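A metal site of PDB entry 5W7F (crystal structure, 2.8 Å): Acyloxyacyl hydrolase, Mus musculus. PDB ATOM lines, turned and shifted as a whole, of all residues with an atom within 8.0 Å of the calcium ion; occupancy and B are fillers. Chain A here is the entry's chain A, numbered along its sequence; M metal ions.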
ATOM      1  N   CYS A 193     -21.413  23.275  -5.759  1.00  0.00           N
ATOM      2  CA  CYS A 193     -21.495  24.726  -5.888  1.00  0.00           C
ATOM      3  C   CYS A 193     -22.428  25.144  -7.009  1.00  0.00           C
ATOM      4  O   CYS A 193     -23.114  26.169  -6.899  1.00  0.00           O
ATOM      5  CB  CYS A 193     -20.103  25.321  -6.105  1.00  0.00           C
ATOM      6  SG  CYS A 193     -19.159  24.567  -7.460  1.00  0.00           S
ATOM      7  N   ARG A 204     -13.501  16.833 -10.016  1.00  0.00           N
ATOM      8  CA  ARG A 204     -13.422  16.932 -11.465  1.00  0.00           C
ATOM      9  C   ARG A 204     -12.097  17.523 -11.906  1.00  0.00           C
ATOM     10  O   ARG A 204     -11.532  18.406 -11.253  1.00  0.00           O
ATOM     11  CB  ARG A 204     -14.573  17.795 -11.997  1.00  0.00           C
ATOM     12  CG  ARG A 204     -14.388  18.266 -13.433  1.00  0.00           C
ATOM     13  CD  ARG A 204     -15.721  18.542 -14.118  1.00  0.00           C
ATOM     14  NE  ARG A 204     -15.567  19.245 -15.384  1.00  0.00           N
ATOM     15  CZ  ARG A 204     -15.123  18.691 -16.516  1.00  0.00           C
ATOM     16  NH1 ARG A 204     -14.769  17.416 -16.534  1.00  0.00           N
ATOM     17  NH2 ARG A 204     -15.023  19.412 -17.620  1.00  0.00           N
ATOM     18  N   ARG A 205     -11.607  17.037 -13.044  1.00  0.00           N
ATOM     19  CA  ARG A 205     -10.433  17.636 -13.654  1.00  0.00           C
ATOM     20  C   ARG A 205     -10.714  19.082 -14.034  1.00  0.00           C
ATOM     21  O   ARG A 205     -11.817  19.401 -14.500  1.00  0.00           O
ATOM     22  CB  ARG A 205      -9.997  16.851 -14.893  1.00  0.00           C
ATOM     23  CG  ARG A 205      -8.901  15.819 -14.666  1.00  0.00           C
ATOM     24  CD  ARG A 205      -8.650  15.015 -15.928  1.00  0.00           C
ATOM     25  NE  ARG A 205      -7.449  14.192 -15.843  1.00  0.00           N
ATOM     26  CZ  ARG A 205      -7.045  13.358 -16.794  1.00  0.00           C
ATOM     27  NH1 ARG A 205      -7.755  13.229 -17.910  1.00  0.00           N
ATOM     28  NH2 ARG A 205      -5.931  12.653 -16.645  1.00  0.00           N
ATOM     29  N   PRO A 206      -9.758  19.995 -13.869  1.00  0.00           N
ATOM     30  CA  PRO A 206     -10.033  21.414 -14.147  1.00  0.00           C
ATOM     31  C   PRO A 206     -10.385  21.622 -15.612  1.00  0.00           C
ATOM     32  O   PRO A 206      -9.606  21.291 -16.512  1.00  0.00           O
ATOM     33  CB  PRO A 206      -8.718  22.106 -13.773  1.00  0.00           C
ATOM     34  CG  PRO A 206      -8.031  21.164 -12.857  1.00  0.00           C
ATOM     35  CD  PRO A 206      -8.410  19.805 -13.315  1.00  0.00           C
ATOM     36  N   ASP A 207     -11.578  22.167 -15.853  1.00  0.00           N
ATOM     37  CA  ASP A 207     -12.035  22.463 -17.208  1.00  0.00           C
ATOM     38  C   ASP A 207     -11.456  23.807 -17.607  1.00  0.00           C
ATOM     39  O   ASP A 207     -11.930  24.865 -17.176  1.00  0.00           O
ATOM     40  CB  ASP A 207     -13.562  22.469 -17.268  1.00  0.00           C
ATOM     41  CG  ASP A 207     -14.087  22.744 -18.664  1.00  0.00           C
ATOM     42  OD1 ASP A 207     -14.547  21.790 -19.324  1.00  0.00           O
ATOM     43  OD2 ASP A 207     -14.039  23.909 -19.100  1.00  0.00           O
ATOM     44  N   TRP A 209      -9.046  24.938 -16.430  1.00  0.00           N
ATOM     45  CA  TRP A 209      -8.554  25.437 -15.150  1.00  0.00           C
ATOM     46  C   TRP A 209      -9.385  26.616 -14.639  1.00  0.00           C
ATOM     47  O   TRP A 209      -8.843  27.589 -14.102  1.00  0.00           O
ATOM     48  CB  TRP A 209      -7.067  25.781 -15.250  1.00  0.00           C
ATOM     49  CG  TRP A 209      -6.251  24.543 -15.497  1.00  0.00           C
ATOM     50  CD1 TRP A 209      -5.653  23.758 -14.554  1.00  0.00           C
ATOM     51  CD2 TRP A 209      -5.978  23.936 -16.767  1.00  0.00           C
ATOM     52  NE1 TRP A 209      -5.017  22.703 -15.152  1.00  0.00           N
ATOM     53  CE2 TRP A 209      -5.202  22.783 -16.514  1.00  0.00           C
ATOM     54  CE3 TRP A 209      -6.302  24.249 -18.080  1.00  0.00           C
ATOM     55  CZ2 TRP A 209      -4.746  21.955 -17.530  1.00  0.00           C
ATOM     56  CZ3 TRP A 209      -5.846  23.421 -19.096  1.00  0.00           C
ATOM     57  CH2 TRP A 209      -5.082  22.286 -18.814  1.00  0.00           C
ATOM     58  N   ASP A 210     -10.701  26.513 -14.809  1.00  0.00           N
ATOM     59  CA  ASP A 210     -11.663  27.381 -14.138  1.00  0.00           C
ATOM     60  C   ASP A 210     -11.332  28.858 -14.338  1.00  0.00           C
ATOM     61  O   ASP A 210     -11.133  29.613 -13.395  1.00  0.00           O
ATOM     62  CB  ASP A 210     -11.742  27.037 -12.650  1.00  0.00           C
ATOM     63  CG  ASP A 210     -11.953  25.557 -12.406  1.00  0.00           C
ATOM     64  OD1 ASP A 210     -12.316  24.839 -13.373  1.00  0.00           O
ATOM     65  OD2 ASP A 210     -11.762  25.100 -11.262  1.00  0.00           O
ATOM     66  N   ILE A 211     -11.282  29.253 -15.611  1.00  0.00           N
ATOM     67  CA  ILE A 211     -11.115  30.664 -15.937  1.00  0.00           C
ATOM     68  C   ILE A 211     -12.320  31.468 -15.482  1.00  0.00           C
ATOM     69  O   ILE A 211     -12.186  32.554 -14.905  1.00  0.00           O
ATOM     70  CB  ILE A 211     -10.843  30.839 -17.439  1.00  0.00           C
ATOM     71  CG1 ILE A 211      -9.521  30.163 -17.815  1.00  0.00           C
ATOM     72  CG2 ILE A 211     -10.811  32.317 -17.807  1.00  0.00           C
ATOM     73  CD1 ILE A 211      -9.243  30.118 -19.304  1.00  0.00           C
ATOM     74  N   GLN A 213     -15.644  29.915 -14.041  1.00  0.00           N
ATOM     75  CA  GLN A 213     -16.425  29.398 -12.931  1.00  0.00           C
ATOM     76  C   GLN A 213     -15.751  28.153 -12.372  1.00  0.00           C
ATOM     77  O   GLN A 213     -15.063  27.417 -13.097  1.00  0.00           O
ATOM     78  CB  GLN A 213     -17.864  29.073 -13.352  1.00  0.00           C
ATOM     79  CG  GLN A 213     -18.903  29.330 -12.262  1.00  0.00           C
ATOM     80  CD  GLN A 213     -20.330  29.208 -12.778  1.00  0.00           C
ATOM     81  OE1 GLN A 213     -20.576  28.610 -13.828  1.00  0.00           O
ATOM     82  NE2 GLN A 213     -21.277  29.775 -12.042  1.00  0.00           N
ATOM     83  N   ASP A 214     -15.938  27.932 -11.069  1.00  0.00           N
ATOM     84  CA  ASP A 214     -15.299  26.814 -10.388  1.00  0.00           C
ATOM     85  C   ASP A 214     -15.878  25.491 -10.895  1.00  0.00           C
ATOM     86  O   ASP A 214     -17.083  25.246 -10.768  1.00  0.00           O
ATOM     87  CB  ASP A 214     -15.495  26.941  -8.881  1.00  0.00           C
ATOM     88  CG  ASP A 214     -14.423  26.215  -8.083  1.00  0.00           C
ATOM     89  OD1 ASP A 214     -14.256  26.532  -6.893  1.00  0.00           O
ATOM     90  OD2 ASP A 214     -13.739  25.344  -8.655  1.00  0.00           O
ATOM     91  N   SER A 215     -15.019  24.652 -11.474  1.00  0.00           N
ATOM     92  CA  SER A 215     -15.481  23.411 -12.091  1.00  0.00           C
ATOM     93  C   SER A 215     -15.638  22.294 -11.062  1.00  0.00           C
ATOM     94  O   SER A 215     -16.565  21.484 -11.181  1.00  0.00           O
ATOM     95  CB  SER A 215     -14.501  22.978 -13.188  1.00  0.00           C
ATOM     96  OG  SER A 215     -13.203  22.753 -12.654  1.00  0.00           O
ATOM     97  N   ASN A 216     -14.765  22.232 -10.065  1.00  0.00           N
ATOM     98  CA  ASN A 216     -14.775  21.160  -9.076  1.00  0.00           C
ATOM     99  C   ASN A 216     -15.118  21.663  -7.672  1.00  0.00           C
ATOM    100  O   ASN A 216     -14.769  21.011  -6.682  1.00  0.00           O
ATOM    101  CB  ASN A 216     -13.429  20.434  -9.071  1.00  0.00           C
ATOM    102  CG  ASN A 216     -12.256  21.385  -9.122  1.00  0.00           C
ATOM    103  OD1 ASN A 216     -12.372  22.550  -8.761  1.00  0.00           O
ATOM    104  ND2 ASN A 216     -11.114  20.881  -9.590  1.00  0.00           N
ATOM    105  N   CYS A 217     -15.792  22.808  -7.568  1.00  0.00           N
ATOM    106  CA  CYS A 217     -16.270  23.349  -6.291  1.00  0.00           C
ATOM    107  C   CYS A 217     -15.203  23.326  -5.205  1.00  0.00           C
ATOM    108  O   CYS A 217     -15.526  23.345  -4.017  1.00  0.00           O
ATOM    109  CB  CYS A 217     -17.516  22.593  -5.810  1.00  0.00           C
ATOM    110  SG  CYS A 217     -18.936  22.627  -6.931  1.00  0.00           S
ATOM    111  N   ASN A 218     -13.918  23.280  -5.573  1.00  0.00           N
ATOM    112  CA  ASN A 218     -12.854  23.248  -4.578  1.00  0.00           C
ATOM    113  C   ASN A 218     -12.427  24.645  -4.147  1.00  0.00           C
ATOM    114  O   ASN A 218     -11.385  24.789  -3.492  1.00  0.00           O
ATOM    115  CB  ASN A 218     -11.648  22.465  -5.111  1.00  0.00           C
ATOM    116  CG  ASN A 218     -10.707  23.320  -5.932  1.00  0.00           C
ATOM    117  OD1 ASN A 218     -11.124  24.214  -6.661  1.00  0.00           O
ATOM    118  ND2 ASN A 218      -9.411  23.052  -5.785  1.00  0.00           N
ATOM    119  N   GLY A 219     -13.203  25.667  -4.499  1.00  0.00           N
ATOM    120  CA  GLY A 219     -12.982  27.018  -4.003  1.00  0.00           C
ATOM    121  C   GLY A 219     -11.904  27.798  -4.705  1.00  0.00           C
ATOM    122  O   GLY A 219     -11.634  28.938  -4.301  1.00  0.00           O
ATOM    123  N   ILE A 220     -11.270  27.250  -5.732  1.00  0.00           N
ATOM    124  CA  ILE A 220     -10.191  27.921  -6.460  1.00  0.00           C
ATOM    125  C   ILE A 220     -10.688  28.178  -7.881  1.00  0.00           C
ATOM    126  O   ILE A 220     -11.077  27.244  -8.586  1.00  0.00           O
ATOM    127  CB  ILE A 220      -8.897  27.092  -6.450  1.00  0.00           C
ATOM    128  CG1 ILE A 220      -8.414  26.903  -5.009  1.00  0.00           C
ATOM    129  CG2 ILE A 220      -7.823  27.780  -7.307  1.00  0.00           C
ATOM    130  CD1 ILE A 220      -7.149  26.080  -4.868  1.00  0.00           C
ATOM    131  N   TRP A 221     -10.667  29.440  -8.287  1.00  0.00           N
ATOM    132  CA  TRP A 221     -11.061  29.817  -9.645  1.00  0.00           C
ATOM    133  C   TRP A 221     -10.497  31.202  -9.918  1.00  0.00           C
ATOM    134  O   TRP A 221      -9.953  31.867  -9.027  1.00  0.00           O
ATOM    135  CB  TRP A 221     -12.585  29.785  -9.801  1.00  0.00           C
ATOM    136  CG  TRP A 221     -13.301  30.899  -9.077  1.00  0.00           C
ATOM    137  CD1 TRP A 221     -13.641  30.931  -7.760  1.00  0.00           C
ATOM    138  CD2 TRP A 221     -13.784  32.126  -9.646  1.00  0.00           C
ATOM    139  NE1 TRP A 221     -14.304  32.101  -7.467  1.00  0.00           N
ATOM    140  CE2 TRP A 221     -14.401  32.851  -8.614  1.00  0.00           C
ATOM    141  CE3 TRP A 221     -13.749  32.677 -10.931  1.00  0.00           C
ATOM    142  CZ2 TRP A 221     -14.971  34.103  -8.818  1.00  0.00           C
ATOM    143  CZ3 TRP A 221     -14.321  33.915 -11.134  1.00  0.00           C
ATOM    144  CH2 TRP A 221     -14.925  34.620 -10.084  1.00  0.00           C
ATOM    145  N   GLY A 222     -10.619  31.632 -11.161  1.00  0.00           N
ATOM    146  CA  GLY A 222     -10.165  32.954 -11.561  1.00  0.00           C
ATOM    147  C   GLY A 222      -8.765  32.923 -12.149  1.00  0.00           C
ATOM    148  O   GLY A 222      -8.207  31.881 -12.504  1.00  0.00           O
ATOM    149  N   TYR A 231      -5.653  30.887 -11.728  1.00  0.00           N
ATOM    150  CA  TYR A 231      -5.287  30.542 -10.347  1.00  0.00           C
ATOM    151  C   TYR A 231      -5.114  29.032 -10.182  1.00  0.00           C
ATOM    152  O   TYR A 231      -4.184  28.588  -9.497  1.00  0.00           O
ATOM    153  CB  TYR A 231      -6.358  31.067  -9.381  1.00  0.00           C
ATOM    154  CG  TYR A 231      -6.100  32.456  -8.835  1.00  0.00           C
ATOM    155  CD1 TYR A 231      -7.115  33.390  -8.776  1.00  0.00           C
ATOM    156  CD2 TYR A 231      -4.845  32.820  -8.354  1.00  0.00           C
ATOM    157  CE1 TYR A 231      -6.899  34.656  -8.272  1.00  0.00           C
ATOM    158  CE2 TYR A 231      -4.616  34.078  -7.851  1.00  0.00           C
ATOM    159  CZ  TYR A 231      -5.642  34.997  -7.801  1.00  0.00           C
ATOM    160  OH  TYR A 231      -5.414  36.256  -7.298  1.00  0.00           O
ATOM    161  N   GLU A 232      -6.001  28.237 -10.786  1.00  0.00           N
ATOM    162  CA  GLU A 232      -6.000  26.798 -10.583  1.00  0.00           C
ATOM    163  C   GLU A 232      -4.661  26.189 -10.996  1.00  0.00           C
ATOM    164  O   GLU A 232      -3.926  25.679 -10.141  1.00  0.00           O
ATOM    165  CB  GLU A 232      -7.149  26.150 -11.367  1.00  0.00           C
ATOM    166  CG  GLU A 232      -7.320  24.654 -11.120  1.00  0.00           C
ATOM    167  CD  GLU A 232      -8.096  24.344  -9.843  1.00  0.00           C
ATOM    168  OE1 GLU A 232      -7.744  23.358  -9.156  1.00  0.00           O
ATOM    169  OE2 GLU A 232      -9.036  25.099  -9.521  1.00  0.00           O
ATOM    170  N   LYS A 233      -4.334  26.223 -12.294  1.00  0.00           N
ATOM    171  CA  LYS A 233      -3.115  25.581 -12.759  1.00  0.00           C
ATOM    172  C   LYS A 233      -1.888  26.177 -12.091  1.00  0.00           C
ATOM    173  O   LYS A 233      -0.916  25.478 -11.814  1.00  0.00           O
ATOM    174  CB  LYS A 233      -2.994  25.698 -14.284  1.00  0.00           C
ATOM    175  CG  LYS A 233      -2.259  24.527 -14.918  1.00  0.00           C
ATOM    176  CD  LYS A 233      -2.320  24.578 -16.439  1.00  0.00           C
ATOM    177  CE  LYS A 233      -1.699  23.327 -17.081  1.00  0.00           C
ATOM    178  NZ  LYS A 233      -1.860  22.084 -16.263  1.00  0.00           N
ATOM    179  N   CYS A 236      -2.495  24.339  -8.317  1.00  0.00           N
ATOM    180  CA  CYS A 236      -2.786  22.923  -8.127  1.00  0.00           C
ATOM    181  C   CYS A 236      -2.135  21.992  -9.134  1.00  0.00           C
ATOM    182  O   CYS A 236      -2.155  20.774  -8.930  1.00  0.00           O
ATOM    183  CB  CYS A 236      -4.309  22.703  -8.162  1.00  0.00           C
ATOM    184  SG  CYS A 236      -5.125  23.292  -6.666  1.00  0.00           S
ATOM    185  N   CYS A 316      -5.799  21.496  -2.642  1.00  0.00           N
ATOM    186  CA  CYS A 316      -6.541  21.203  -3.858  1.00  0.00           C
ATOM    187  C   CYS A 316      -7.554  20.080  -3.647  1.00  0.00           C
ATOM    188  O   CYS A 316      -8.603  20.065  -4.300  1.00  0.00           O
ATOM    189  CB  CYS A 316      -5.570  20.847  -4.977  1.00  0.00           C
ATOM    190  SG  CYS A 316      -4.316  22.115  -5.230  1.00  0.00           S
ATOM    191  N   GLN A 559     -12.006  28.929   1.338  1.00  0.00           N
ATOM    192  CA  GLN A 559     -12.385  28.344   0.046  1.00  0.00           C
ATOM    193  C   GLN A 559     -13.868  28.007  -0.001  1.00  0.00           C
ATOM    194  O   GLN A 559     -14.268  26.995  -0.569  1.00  0.00           O
ATOM    195  CB  GLN A 559     -11.538  27.106  -0.257  1.00  0.00           C
ATOM    196  CG  GLN A 559     -10.057  27.283  -0.021  1.00  0.00           C
ATOM    197  CD  GLN A 559      -9.249  26.072  -0.432  1.00  0.00           C
ATOM    198  OE1 GLN A 559      -9.574  25.401  -1.408  1.00  0.00           O
ATOM    199  NE2 GLN A 559      -8.186  25.783   0.317  1.00  0.00           N
HETATM  200 CA    CA M   1     -11.457  24.886  -8.992  1.00  0.00          CA
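The backbone NH (N) of Ser 215 lies close to the side-chain carboxylate (OD1) of Asp 210 (3.3 Å). O of Asp 210 sits at hydrogen-bond distance from N of Gly 222, at 3.1 Å. The side-chain carboxylate (OD1) of Asp 214 sits at hydrogen-bond distance from the backbone NH (N) of Gly 219 (2.8 Å). OD2 of Asp 214 sits close to N of Cys 217, 3.4 Å away. ND2 of Asn 218 lies within hydrogen-bond range of O of Cys 316, 3.4 Å away. The backbone carbonyl oxygen (O) of Asn 218 lies close to the side-chain amide oxygen (OE1) of Gln 559 (2.8 Å). SG of Cys 217 forms a disulfide with SG of Cys 193. SG of Cys 236 is disulfide-bonded to SG of Cys 316 (2.0 Å).
The calcium ion is bound by the side-chain carboxylate (OD2) of Asp 210 (2.3 Å), the side-chain carboxylate (OD2) of Asp 214 (2.4 Å), the backbone carbonyl oxygen (O) of Ile 220 (2.4 Å), the side-chain amide oxygen (OD1) of Asn 218 (2.4 Å), the side-chain carboxylate (OE2) of Glu 232 (2.5 Å) and the side-chain amide oxygen (OD1) of Asn 216 (2.5 Å).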
